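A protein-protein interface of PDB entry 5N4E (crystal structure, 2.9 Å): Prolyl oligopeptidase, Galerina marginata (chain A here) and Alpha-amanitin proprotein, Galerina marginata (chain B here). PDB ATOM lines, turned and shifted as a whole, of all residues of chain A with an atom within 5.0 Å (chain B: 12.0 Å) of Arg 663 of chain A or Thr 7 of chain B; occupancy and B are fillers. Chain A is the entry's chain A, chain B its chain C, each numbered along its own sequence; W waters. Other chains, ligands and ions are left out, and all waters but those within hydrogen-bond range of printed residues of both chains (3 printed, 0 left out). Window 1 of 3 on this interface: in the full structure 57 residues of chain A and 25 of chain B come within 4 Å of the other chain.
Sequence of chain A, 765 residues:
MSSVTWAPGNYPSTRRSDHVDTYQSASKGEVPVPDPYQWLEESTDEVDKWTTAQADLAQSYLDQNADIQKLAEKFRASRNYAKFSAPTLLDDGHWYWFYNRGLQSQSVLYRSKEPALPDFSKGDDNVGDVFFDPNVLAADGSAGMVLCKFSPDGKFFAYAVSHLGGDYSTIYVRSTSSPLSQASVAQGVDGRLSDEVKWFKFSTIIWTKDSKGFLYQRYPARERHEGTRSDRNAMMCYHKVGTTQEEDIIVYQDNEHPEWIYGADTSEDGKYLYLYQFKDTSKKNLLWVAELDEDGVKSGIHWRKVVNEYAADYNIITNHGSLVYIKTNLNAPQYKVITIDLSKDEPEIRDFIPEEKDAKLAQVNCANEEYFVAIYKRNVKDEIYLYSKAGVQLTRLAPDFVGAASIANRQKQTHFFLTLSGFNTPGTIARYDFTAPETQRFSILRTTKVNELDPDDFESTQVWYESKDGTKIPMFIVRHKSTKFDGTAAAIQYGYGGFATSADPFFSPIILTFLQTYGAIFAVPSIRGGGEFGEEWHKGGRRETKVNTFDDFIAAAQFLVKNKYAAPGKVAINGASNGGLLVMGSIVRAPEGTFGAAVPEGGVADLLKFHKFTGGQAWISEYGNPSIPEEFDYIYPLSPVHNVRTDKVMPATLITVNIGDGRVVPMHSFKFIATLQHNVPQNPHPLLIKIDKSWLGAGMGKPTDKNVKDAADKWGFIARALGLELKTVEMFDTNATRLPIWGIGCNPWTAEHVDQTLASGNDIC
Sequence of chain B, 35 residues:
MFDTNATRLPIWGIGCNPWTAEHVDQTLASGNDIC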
ATOM      1  N   PHE A 202      21.189   9.243   9.169  1.00  0.00           N
ATOM      2  CA  PHE A 202      21.919  10.515   9.072  1.00  0.00           C
ATOM      3  C   PHE A 202      20.986  11.726   9.115  1.00  0.00           C
ATOM      4  O   PHE A 202      20.990  12.577   8.222  1.00  0.00           O
ATOM      5  CB  PHE A 202      22.797  10.556   7.811  1.00  0.00           C
ATOM      6  CG  PHE A 202      23.774   9.410   7.689  1.00  0.00           C
ATOM      7  CD1 PHE A 202      24.450   8.901   8.801  1.00  0.00           C
ATOM      8  CD2 PHE A 202      24.050   8.862   6.439  1.00  0.00           C
ATOM      9  CE1 PHE A 202      25.356   7.859   8.665  1.00  0.00           C
ATOM     10  CE2 PHE A 202      24.954   7.820   6.301  1.00  0.00           C
ATOM     11  CZ  PHE A 202      25.611   7.322   7.415  1.00  0.00           C
ATOM     12  N   SER A 203      20.184  11.788  10.170  1.00  0.00           N
ATOM     13  CA  SER A 203      19.120  12.775  10.269  1.00  0.00           C
ATOM     14  C   SER A 203      18.631  12.945  11.701  1.00  0.00           C
ATOM     15  O   SER A 203      19.076  12.251  12.616  1.00  0.00           O
ATOM     16  CB  SER A 203      17.964  12.352   9.357  1.00  0.00           C
ATOM     17  OG  SER A 203      16.856  13.232   9.428  1.00  0.00           O
ATOM     18  N   THR A 614      30.663   1.602   1.946  1.00  0.00           N
ATOM     19  CA  THR A 614      29.573   2.313   2.656  1.00  0.00           C
ATOM     20  C   THR A 614      29.594   3.847   2.444  1.00  0.00           C
ATOM     21  O   THR A 614      29.540   4.287   1.296  1.00  0.00           O
ATOM     22  CB  THR A 614      29.514   1.924   4.157  1.00  0.00           C
ATOM     23  OG1 THR A 614      30.616   2.519   4.849  1.00  0.00           O
ATOM     24  CG2 THR A 614      29.517   0.417   4.345  1.00  0.00           C
ATOM     25  N   TRP A 619      34.162  11.213   2.789  1.00  0.00           N
ATOM     26  CA  TRP A 619      35.420  11.573   3.459  1.00  0.00           C
ATOM     27  C   TRP A 619      36.544  11.997   2.504  1.00  0.00           C
ATOM     28  O   TRP A 619      37.634  12.343   2.965  1.00  0.00           O
ATOM     29  CB  TRP A 619      35.920  10.433   4.358  1.00  0.00           C
ATOM     30  CG  TRP A 619      34.885   9.846   5.274  1.00  0.00           C
ATOM     31  CD1 TRP A 619      33.777  10.467   5.780  1.00  0.00           C
ATOM     32  CD2 TRP A 619      34.872   8.515   5.798  1.00  0.00           C
ATOM     33  NE1 TRP A 619      33.068   9.599   6.577  1.00  0.00           N
ATOM     34  CE2 TRP A 619      33.720   8.395   6.610  1.00  0.00           C
ATOM     35  CE3 TRP A 619      35.725   7.410   5.663  1.00  0.00           C
ATOM     36  CZ2 TRP A 619      33.399   7.215   7.282  1.00  0.00           C
ATOM     37  CZ3 TRP A 619      35.405   6.234   6.327  1.00  0.00           C
ATOM     38  CH2 TRP A 619      34.251   6.148   7.129  1.00  0.00           C
ATOM     39  N   ASP A 661      30.508  -2.983  12.426  1.00  0.00           N
ATOM     40  CA  ASP A 661      30.678  -1.543  12.207  1.00  0.00           C
ATOM     41  C   ASP A 661      30.432  -1.220  10.730  1.00  0.00           C
ATOM     42  O   ASP A 661      31.184  -1.663   9.854  1.00  0.00           O
ATOM     43  CB  ASP A 661      32.088  -1.097  12.637  1.00  0.00           C
ATOM     44  CG  ASP A 661      32.243   0.423  12.745  1.00  0.00           C
ATOM     45  OD1 ASP A 661      31.364   1.186  12.288  1.00  0.00           O
ATOM     46  OD2 ASP A 661      33.277   0.860  13.299  1.00  0.00           O
ATOM     47  N   GLY A 662      29.364  -0.467  10.474  1.00  0.00           N
ATOM     48  CA  GLY A 662      29.017   0.002   9.133  1.00  0.00           C
ATOM     49  C   GLY A 662      29.571   1.372   8.772  1.00  0.00           C
ATOM     50  O   GLY A 662      29.600   1.726   7.589  1.00  0.00           O
ATOM     51  N   ARG A 663      30.005   2.146   9.771  1.00  0.00           N
ATOM     52  CA  ARG A 663      30.589   3.472   9.532  1.00  0.00           C
ATOM     53  C   ARG A 663      31.980   3.305   8.919  1.00  0.00           C
ATOM     54  O   ARG A 663      32.211   3.719   7.783  1.00  0.00           O
ATOM     55  CB  ARG A 663      30.682   4.287  10.826  1.00  0.00           C
ATOM     56  CG  ARG A 663      29.360   4.573  11.503  1.00  0.00           C
ATOM     57  CD  ARG A 663      28.551   5.612  10.750  1.00  0.00           C
ATOM     58  NE  ARG A 663      27.618   6.296  11.651  1.00  0.00           N
ATOM     59  CZ  ARG A 663      27.948   7.246  12.533  1.00  0.00           C
ATOM     60  NH1 ARG A 663      29.208   7.671  12.663  1.00  0.00           N
ATOM     61  NH2 ARG A 663      27.000   7.780  13.300  1.00  0.00           N
ATOM     62  N   VAL A 664      32.885   2.681   9.677  1.00  0.00           N
ATOM     63  CA  VAL A 664      34.225   2.335   9.215  1.00  0.00           C
ATOM     64  C   VAL A 664      34.273   0.817   9.176  1.00  0.00           C
ATOM     65  O   VAL A 664      34.301   0.166  10.224  1.00  0.00           O
ATOM     66  CB  VAL A 664      35.327   2.864  10.170  1.00  0.00           C
ATOM     67  CG1 VAL A 664      36.716   2.474   9.671  1.00  0.00           C
ATOM     68  CG2 VAL A 664      35.228   4.374  10.317  1.00  0.00           C
ATOM     69  N   VAL A 665      34.255   0.253   7.969  1.00  0.00           N
ATOM     70  CA  VAL A 665      34.307  -1.205   7.799  1.00  0.00           C
ATOM     71  C   VAL A 665      35.560  -1.798   8.473  1.00  0.00           C
ATOM     72  O   VAL A 665      36.646  -1.233   8.350  1.00  0.00           O
ATOM     73  CB  VAL A 665      34.213  -1.649   6.311  1.00  0.00           C
ATOM     74  CG1 VAL A 665      32.803  -1.414   5.779  1.00  0.00           C
ATOM     75  CG2 VAL A 665      35.249  -0.958   5.421  1.00  0.00           C
ATOM     76  N   PHE B   2      22.246  19.842  16.989  1.00  0.00           N
ATOM     77  CA  PHE B   2      22.395  18.736  15.988  1.00  0.00           C
ATOM     78  C   PHE B   2      23.098  19.221  14.719  1.00  0.00           C
ATOM     79  O   PHE B   2      22.893  20.355  14.278  1.00  0.00           O
ATOM     80  CB  PHE B   2      21.026  18.139  15.637  1.00  0.00           C
ATOM     81  CG  PHE B   2      21.097  16.915  14.759  1.00  0.00           C
ATOM     82  CD1 PHE B   2      21.350  15.662  15.309  1.00  0.00           C
ATOM     83  CD2 PHE B   2      20.904  17.014  13.382  1.00  0.00           C
ATOM     84  CE1 PHE B   2      21.410  14.532  14.505  1.00  0.00           C
ATOM     85  CE2 PHE B   2      20.968  15.889  12.573  1.00  0.00           C
ATOM     86  CZ  PHE B   2      21.221  14.647  13.135  1.00  0.00           C
ATOM     87  N   ASP B   3      23.929  18.349  14.152  1.00  0.00           N
ATOM     88  CA  ASP B   3      24.629  18.597  12.894  1.00  0.00           C
ATOM     89  C   ASP B   3      24.400  17.369  12.010  1.00  0.00           C
ATOM     90  O   ASP B   3      24.847  16.271  12.346  1.00  0.00           O
ATOM     91  CB  ASP B   3      26.121  18.833  13.173  1.00  0.00           C
ATOM     92  CG  ASP B   3      26.905  19.303  11.944  1.00  0.00           C
ATOM     93  OD1 ASP B   3      26.365  19.304  10.818  1.00  0.00           O
ATOM     94  OD2 ASP B   3      28.087  19.671  12.110  1.00  0.00           O
ATOM     95  N   THR B   4      23.681  17.561  10.902  1.00  0.00           N
ATOM     96  CA  THR B   4      23.346  16.483   9.958  1.00  0.00           C
ATOM     97  C   THR B   4      24.585  15.844   9.341  1.00  0.00           C
ATOM     98  O   THR B   4      24.701  14.617   9.289  1.00  0.00           O
ATOM     99  CB  THR B   4      22.445  17.006   8.815  1.00  0.00           C
ATOM    100  OG1 THR B   4      21.212  17.492   9.360  1.00  0.00           O
ATOM    101  CG2 THR B   4      22.143  15.912   7.783  1.00  0.00           C
ATOM    102  N   ASN B   5      25.498  16.686   8.875  1.00  0.00           N
ATOM    103  CA  ASN B   5      26.714  16.224   8.209  1.00  0.00           C
ATOM    104  C   ASN B   5      27.684  15.528   9.185  1.00  0.00           C
ATOM    105  O   ASN B   5      28.444  14.645   8.776  1.00  0.00           O
ATOM    106  CB  ASN B   5      27.398  17.408   7.497  1.00  0.00           C
ATOM    107  CG  ASN B   5      28.191  16.992   6.267  1.00  0.00           C
ATOM    108  OD1 ASN B   5      28.024  15.896   5.731  1.00  0.00           O
ATOM    109  ND2 ASN B   5      29.052  17.887   5.801  1.00  0.00           N
ATOM    110  N   ALA B   6      27.638  15.913  10.463  1.00  0.00           N
ATOM    111  CA  ALA B   6      28.487  15.314  11.503  1.00  0.00           C
ATOM    112  C   ALA B   6      28.059  13.909  11.951  1.00  0.00           C
ATOM    113  O   ALA B   6      28.851  13.198  12.576  1.00  0.00           O
ATOM    114  CB  ALA B   6      28.582  16.229  12.713  1.00  0.00           C
ATOM    115  N   THR B   7      26.821  13.510  11.646  1.00  0.00           N
ATOM    116  CA  THR B   7      26.325  12.166  11.993  1.00  0.00           C
ATOM    117  C   THR B   7      26.928  11.038  11.146  1.00  0.00           C
ATOM    118  O   THR B   7      26.731   9.867  11.476  1.00  0.00           O
ATOM    119  CB  THR B   7      24.787  12.063  11.864  1.00  0.00           C
ATOM    120  OG1 THR B   7      24.395  12.286  10.506  1.00  0.00           O
ATOM    121  CG2 THR B   7      24.090  13.063  12.766  1.00  0.00           C
ATOM    122  N   ARG B   8      27.628  11.386  10.061  1.00  0.00           N
ATOM    123  CA  ARG B   8      28.266  10.407   9.172  1.00  0.00           C
ATOM    124  C   ARG B   8      29.802  10.528   9.129  1.00  0.00           C
ATOM    125  O   ARG B   8      30.438  10.004   8.212  1.00  0.00           O
ATOM    126  CB  ARG B   8      27.667  10.518   7.763  1.00  0.00           C
ATOM    127  CG  ARG B   8      27.806  11.881   7.102  1.00  0.00           C
ATOM    128  CD  ARG B   8      27.416  11.808   5.638  1.00  0.00           C
ATOM    129  NE  ARG B   8      27.533  13.106   4.978  1.00  0.00           N
ATOM    130  CZ  ARG B   8      27.482  13.304   3.659  1.00  0.00           C
ATOM    131  NH1 ARG B   8      27.314  12.290   2.810  1.00  0.00           N
ATOM    132  NH2 ARG B   8      27.603  14.538   3.177  1.00  0.00           N
ATOM    133  N   LEU B   9      30.390  11.198  10.126  1.00  0.00           N
ATOM    134  CA  LEU B   9      31.844  11.289  10.241  1.00  0.00           C
ATOM    135  C   LEU B   9      32.407   9.956  10.714  1.00  0.00           C
ATOM    136  O   LEU B   9      31.686   9.172  11.344  1.00  0.00           O
ATOM    137  CB  LEU B   9      32.251  12.352  11.267  1.00  0.00           C
ATOM    138  CG  LEU B   9      31.839  13.797  11.036  1.00  0.00           C
ATOM    139  CD1 LEU B   9      32.319  14.654  12.201  1.00  0.00           C
ATOM    140  CD2 LEU B   9      32.392  14.310   9.719  1.00  0.00           C
ATOM    141  N   PRO B  10      33.703   9.700  10.437  1.00  0.00           N
ATOM    142  CA  PRO B  10      34.344   8.587  11.118  1.00  0.00           C
ATOM    143  C   PRO B  10      34.668   9.025  12.549  1.00  0.00           C
ATOM    144  O   PRO B  10      35.766   9.504  12.824  1.00  0.00           O
ATOM    145  CB  PRO B  10      35.596   8.325  10.269  1.00  0.00           C
ATOM    146  CG  PRO B  10      35.902   9.624   9.609  1.00  0.00           C
ATOM    147  CD  PRO B  10      34.665  10.483   9.638  1.00  0.00           C
ATOM    148  N   ILE B  11      33.685   8.859  13.435  1.00  0.00           N
ATOM    149  CA  ILE B  11      33.765   9.265  14.846  1.00  0.00           C
ATOM    150  C   ILE B  11      33.076   8.201  15.708  1.00  0.00           C
ATOM    151  O   ILE B  11      32.193   7.489  15.218  1.00  0.00           O
ATOM    152  CB  ILE B  11      33.132  10.666  15.062  1.00  0.00           C
ATOM    153  CG1 ILE B  11      33.530  11.251  16.424  1.00  0.00           C
ATOM    154  CG2 ILE B  11      31.611  10.627  14.898  1.00  0.00           C
ATOM    155  CD1 ILE B  11      33.242  12.729  16.563  1.00  0.00           C
ATOM    156  N   TRP B  12      33.476   8.094  16.978  1.00  0.00           N
ATOM    157  CA  TRP B  12      33.027   6.998  17.851  1.00  0.00           C
ATOM    158  C   TRP B  12      31.508   6.915  18.087  1.00  0.00           C
ATOM    159  O   TRP B  12      30.925   5.835  17.901  1.00  0.00           O
ATOM    160  CB  TRP B  12      33.744   7.039  19.205  1.00  0.00           C
ATOM    161  CG  TRP B  12      33.452   5.829  20.051  1.00  0.00           C
ATOM    162  CD1 TRP B  12      34.011   4.593  19.921  1.00  0.00           C
ATOM    163  CD2 TRP B  12      32.516   5.737  21.135  1.00  0.00           C
ATOM    164  NE1 TRP B  12      33.495   3.736  20.864  1.00  0.00           N
ATOM    165  CE2 TRP B  12      32.571   4.409  21.619  1.00  0.00           C
ATOM    166  CE3 TRP B  12      31.637   6.645  21.748  1.00  0.00           C
ATOM    167  CZ2 TRP B  12      31.789   3.965  22.693  1.00  0.00           C
ATOM    168  CZ3 TRP B  12      30.851   6.199  22.816  1.00  0.00           C
ATOM    169  CH2 TRP B  12      30.939   4.870  23.276  1.00  0.00           C
ATOM    170  N   GLY B  13      30.888   8.018  18.493  1.00  0.00           N
ATOM    171  CA  GLY B  13      29.472   7.997  18.879  1.00  0.00           C
ATOM    172  C   GLY B  13      28.841   9.361  19.008  1.00  0.00           C
ATOM    173  O   GLY B  13      29.510  10.332  19.371  1.00  0.00           O
ATOM    174  N   ILE B  14      27.533   9.418  18.732  1.00  0.00           N
ATOM    175  CA  ILE B  14      26.738  10.667  18.778  1.00  0.00           C
ATOM    176  C   ILE B  14      26.053  10.828  20.142  1.00  0.00           C
ATOM    177  O   ILE B  14      24.899  10.449  20.339  1.00  0.00           O
ATOM    178  CB  ILE B  14      25.727  10.773  17.582  1.00  0.00           C
ATOM    179  CG1 ILE B  14      24.820  12.023  17.668  1.00  0.00           C
ATOM    180  CG2 ILE B  14      24.882   9.506  17.406  1.00  0.00           C
ATOM    181  CD1 ILE B  14      25.542  13.346  17.824  1.00  0.00           C
ATOM    182  N   TRP B  19      33.935  12.109  20.662  1.00  0.00           N
ATOM    183  CA  TRP B  19      35.138  11.879  19.851  1.00  0.00           C
ATOM    184  C   TRP B  19      36.091  10.788  20.384  1.00  0.00           C
ATOM    185  O   TRP B  19      37.172  10.595  19.822  1.00  0.00           O
ATOM    186  CB  TRP B  19      35.898  13.204  19.607  1.00  0.00           C
ATOM    187  CG  TRP B  19      36.445  13.886  20.840  1.00  0.00           C
ATOM    188  CD1 TRP B  19      35.779  14.752  21.661  1.00  0.00           C
ATOM    189  CD2 TRP B  19      37.778  13.785  21.363  1.00  0.00           C
ATOM    190  NE1 TRP B  19      36.605  15.180  22.673  1.00  0.00           N
ATOM    191  CE2 TRP B  19      37.838  14.602  22.516  1.00  0.00           C
ATOM    192  CE3 TRP B  19      38.925  13.075  20.976  1.00  0.00           C
ATOM    193  CZ2 TRP B  19      39.003  14.731  23.289  1.00  0.00           C
ATOM    194  CZ3 TRP B  19      40.086  13.199  21.751  1.00  0.00           C
ATOM    195  CH2 TRP B  19      40.112  14.024  22.891  1.00  0.00           C
ATOM    196  N   THR B  20      35.691  10.077  21.446  1.00  0.00           N
ATOM    197  CA  THR B  20      36.500   8.997  22.046  1.00  0.00           C
ATOM    198  C   THR B  20      35.617   7.846  22.526  1.00  0.00           C
ATOM    199  O   THR B  20      34.391   7.967  22.573  1.00  0.00           O
ATOM    200  CB  THR B  20      37.329   9.457  23.277  1.00  0.00           C
ATOM    201  OG1 THR B  20      36.488   9.574  24.428  1.00  0.00           O
ATOM    202  CG2 THR B  20      38.025  10.772  23.047  1.00  0.00           C
ATOM    203  N   GLN B  26      26.448   9.912  27.420  1.00  0.00           N
ATOM    204  CA  GLN B  26      25.971  11.180  26.885  1.00  0.00           C
ATOM    205  C   GLN B  26      24.654  11.622  27.544  1.00  0.00           C
ATOM    206  O   GLN B  26      23.876  12.352  26.934  1.00  0.00           O
ATOM    207  CB  GLN B  26      25.772  11.044  25.364  1.00  0.00           C
ATOM    208  CG  GLN B  26      27.010  10.662  24.556  1.00  0.00           C
ATOM    209  CD  GLN B  26      28.001  11.798  24.420  1.00  0.00           C
ATOM    210  OE1 GLN B  26      29.180  11.657  24.731  1.00  0.00           O
ATOM    211  NE2 GLN B  26      27.524  12.940  23.928  1.00  0.00           N
ATOM    212  N   ASP B  33      17.961  19.010  23.189  1.00  0.00           N
ATOM    213  CA  ASP B  33      17.070  19.280  22.055  1.00  0.00           C
ATOM    214  C   ASP B  33      16.118  18.109  21.776  1.00  0.00           C
ATOM    215  O   ASP B  33      16.228  17.421  20.760  1.00  0.00           O
ATOM    216  CB  ASP B  33      17.896  19.655  20.812  1.00  0.00           C
ATOM    217  CG  ASP B  33      17.053  20.269  19.698  1.00  0.00           C
ATOM    218  OD1 ASP B  33      17.448  20.119  18.524  1.00  0.00           O
ATOM    219  OD2 ASP B  33      16.009  20.898  19.984  1.00  0.00           O
HETATM  220  O   HOH W   1      24.450   8.705  13.137  1.00  0.00           O
HETATM  221  O   HOH W   2      30.119   7.873   6.268  1.00  0.00           O
HETATM  222  O   HOH W   3      28.731  10.310  13.633  1.00  0.00           O
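Of the 9 printed residues of chain A, 5 touch a printed residue of chain B. Hydrophobic or aromatic side chains of chain B within 4 Å of the printed part of chain A: Phe 2 and Pro 10. Among the printed residues, no Asp or Glu carboxylate lies within 4 Å of a Lys or Arg side-chain nitrogen of the other chain.
Among the printed residues, merely in contact across the chains: Phe 202 of chain A with Thr 4 of chain B (3.6 Å), Phe 202 of chain A with Thr 7 of chain B (3.4 Å), Phe 202 of chain A with Arg 8 of chain B (3.6 Å), Ser 203 of chain A with Phe 2 of chain B (3.3 Å), Trp 619 of chain A with Pro 10 of chain B (3.6 Å), Arg 663 of chain A with Ile 11 of chain B (3.9 Å) and Val 664 of chain A with Pro 10 of chain B (3.97 Å).
Of the printed residues of chain B, Phe 202 of chain A touches Thr 4 (3.6 Å), Thr 7 (3.4 Å) and Arg 8 (3.6 Å). No residue of chain B comes within 4 Å of Thr 614 of chain A. No residue of chain B comes within 4 Å of Asp 661 of chain A. Val 664 of chain A touches just one residue of chain B: Pro 10 (3.97 Å). No residue of chain B comes within 4 Å of Val 665 of chain A. Printed residues of chain A within 4 Å of Thr 4 of chain B: Phe 202 (3.6 Å). Thr 7 of chain B touches just these residues of chain A: Phe 202 (3.4 Å) and Arg 663 (2.8 Å). Printed residues of chain A within 4 Å of Leu 9 of chain B: Arg 663.
O of Arg 8 of chain B lies within hydrogen-bond range of NE1 of Trp 619 of chain A (3.1 Å). The backbone carbonyl oxygen (O) of Thr 7 of chain B sits at hydrogen-bond distance from the guanidinium group (NH2) of Arg 663 of chain A, 2.8 Å away. The backbone carbonyl oxygen (O) of Leu 9 of chain B is in hydrogen-bond range of the guanidinium group (NH1) of Arg 663 of chain A (3.2 Å).
Water W1 bridges the guanidinium group (NH2) of Arg 663 of chain A (2.7 Å) and the backbone carbonyl oxygen (O) of Thr 7 of chain B (3.1 Å). Water W3 lies within hydrogen-bond range of the guanidinium group of Arg 663 of chain A (2.9 Å), the backbone carbonyl oxygen of Thr 7 of chain B (3.0 Å) and the backbone carbonyl oxygen of Ala 6 of chain B (3.1 Å). Water W2 bridges O of Arg 8 of chain B (2.9 Å) and NE1 of Trp 619 of chain A (3.4 Å).
N of Arg 663 of chain A is in hydrogen-bond range of OD1 of Asp 661 of chain A (3.0 Å). The side-chain carboxylate (OD1) of Asp 661 of chain A lies within hydrogen-bond range of the backbone NH (N) of Val 664 of chain A. The backbone carbonyl oxygen (O) of Thr 4 of chain B sits at hydrogen-bond distance from the side-chain hydroxyl (OG1) of Thr 7 of chain B, at 2.6 Å. OD1 of Asn 5 of chain B sits at hydrogen-bond distance from NH2 of Arg 8 of chain B.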
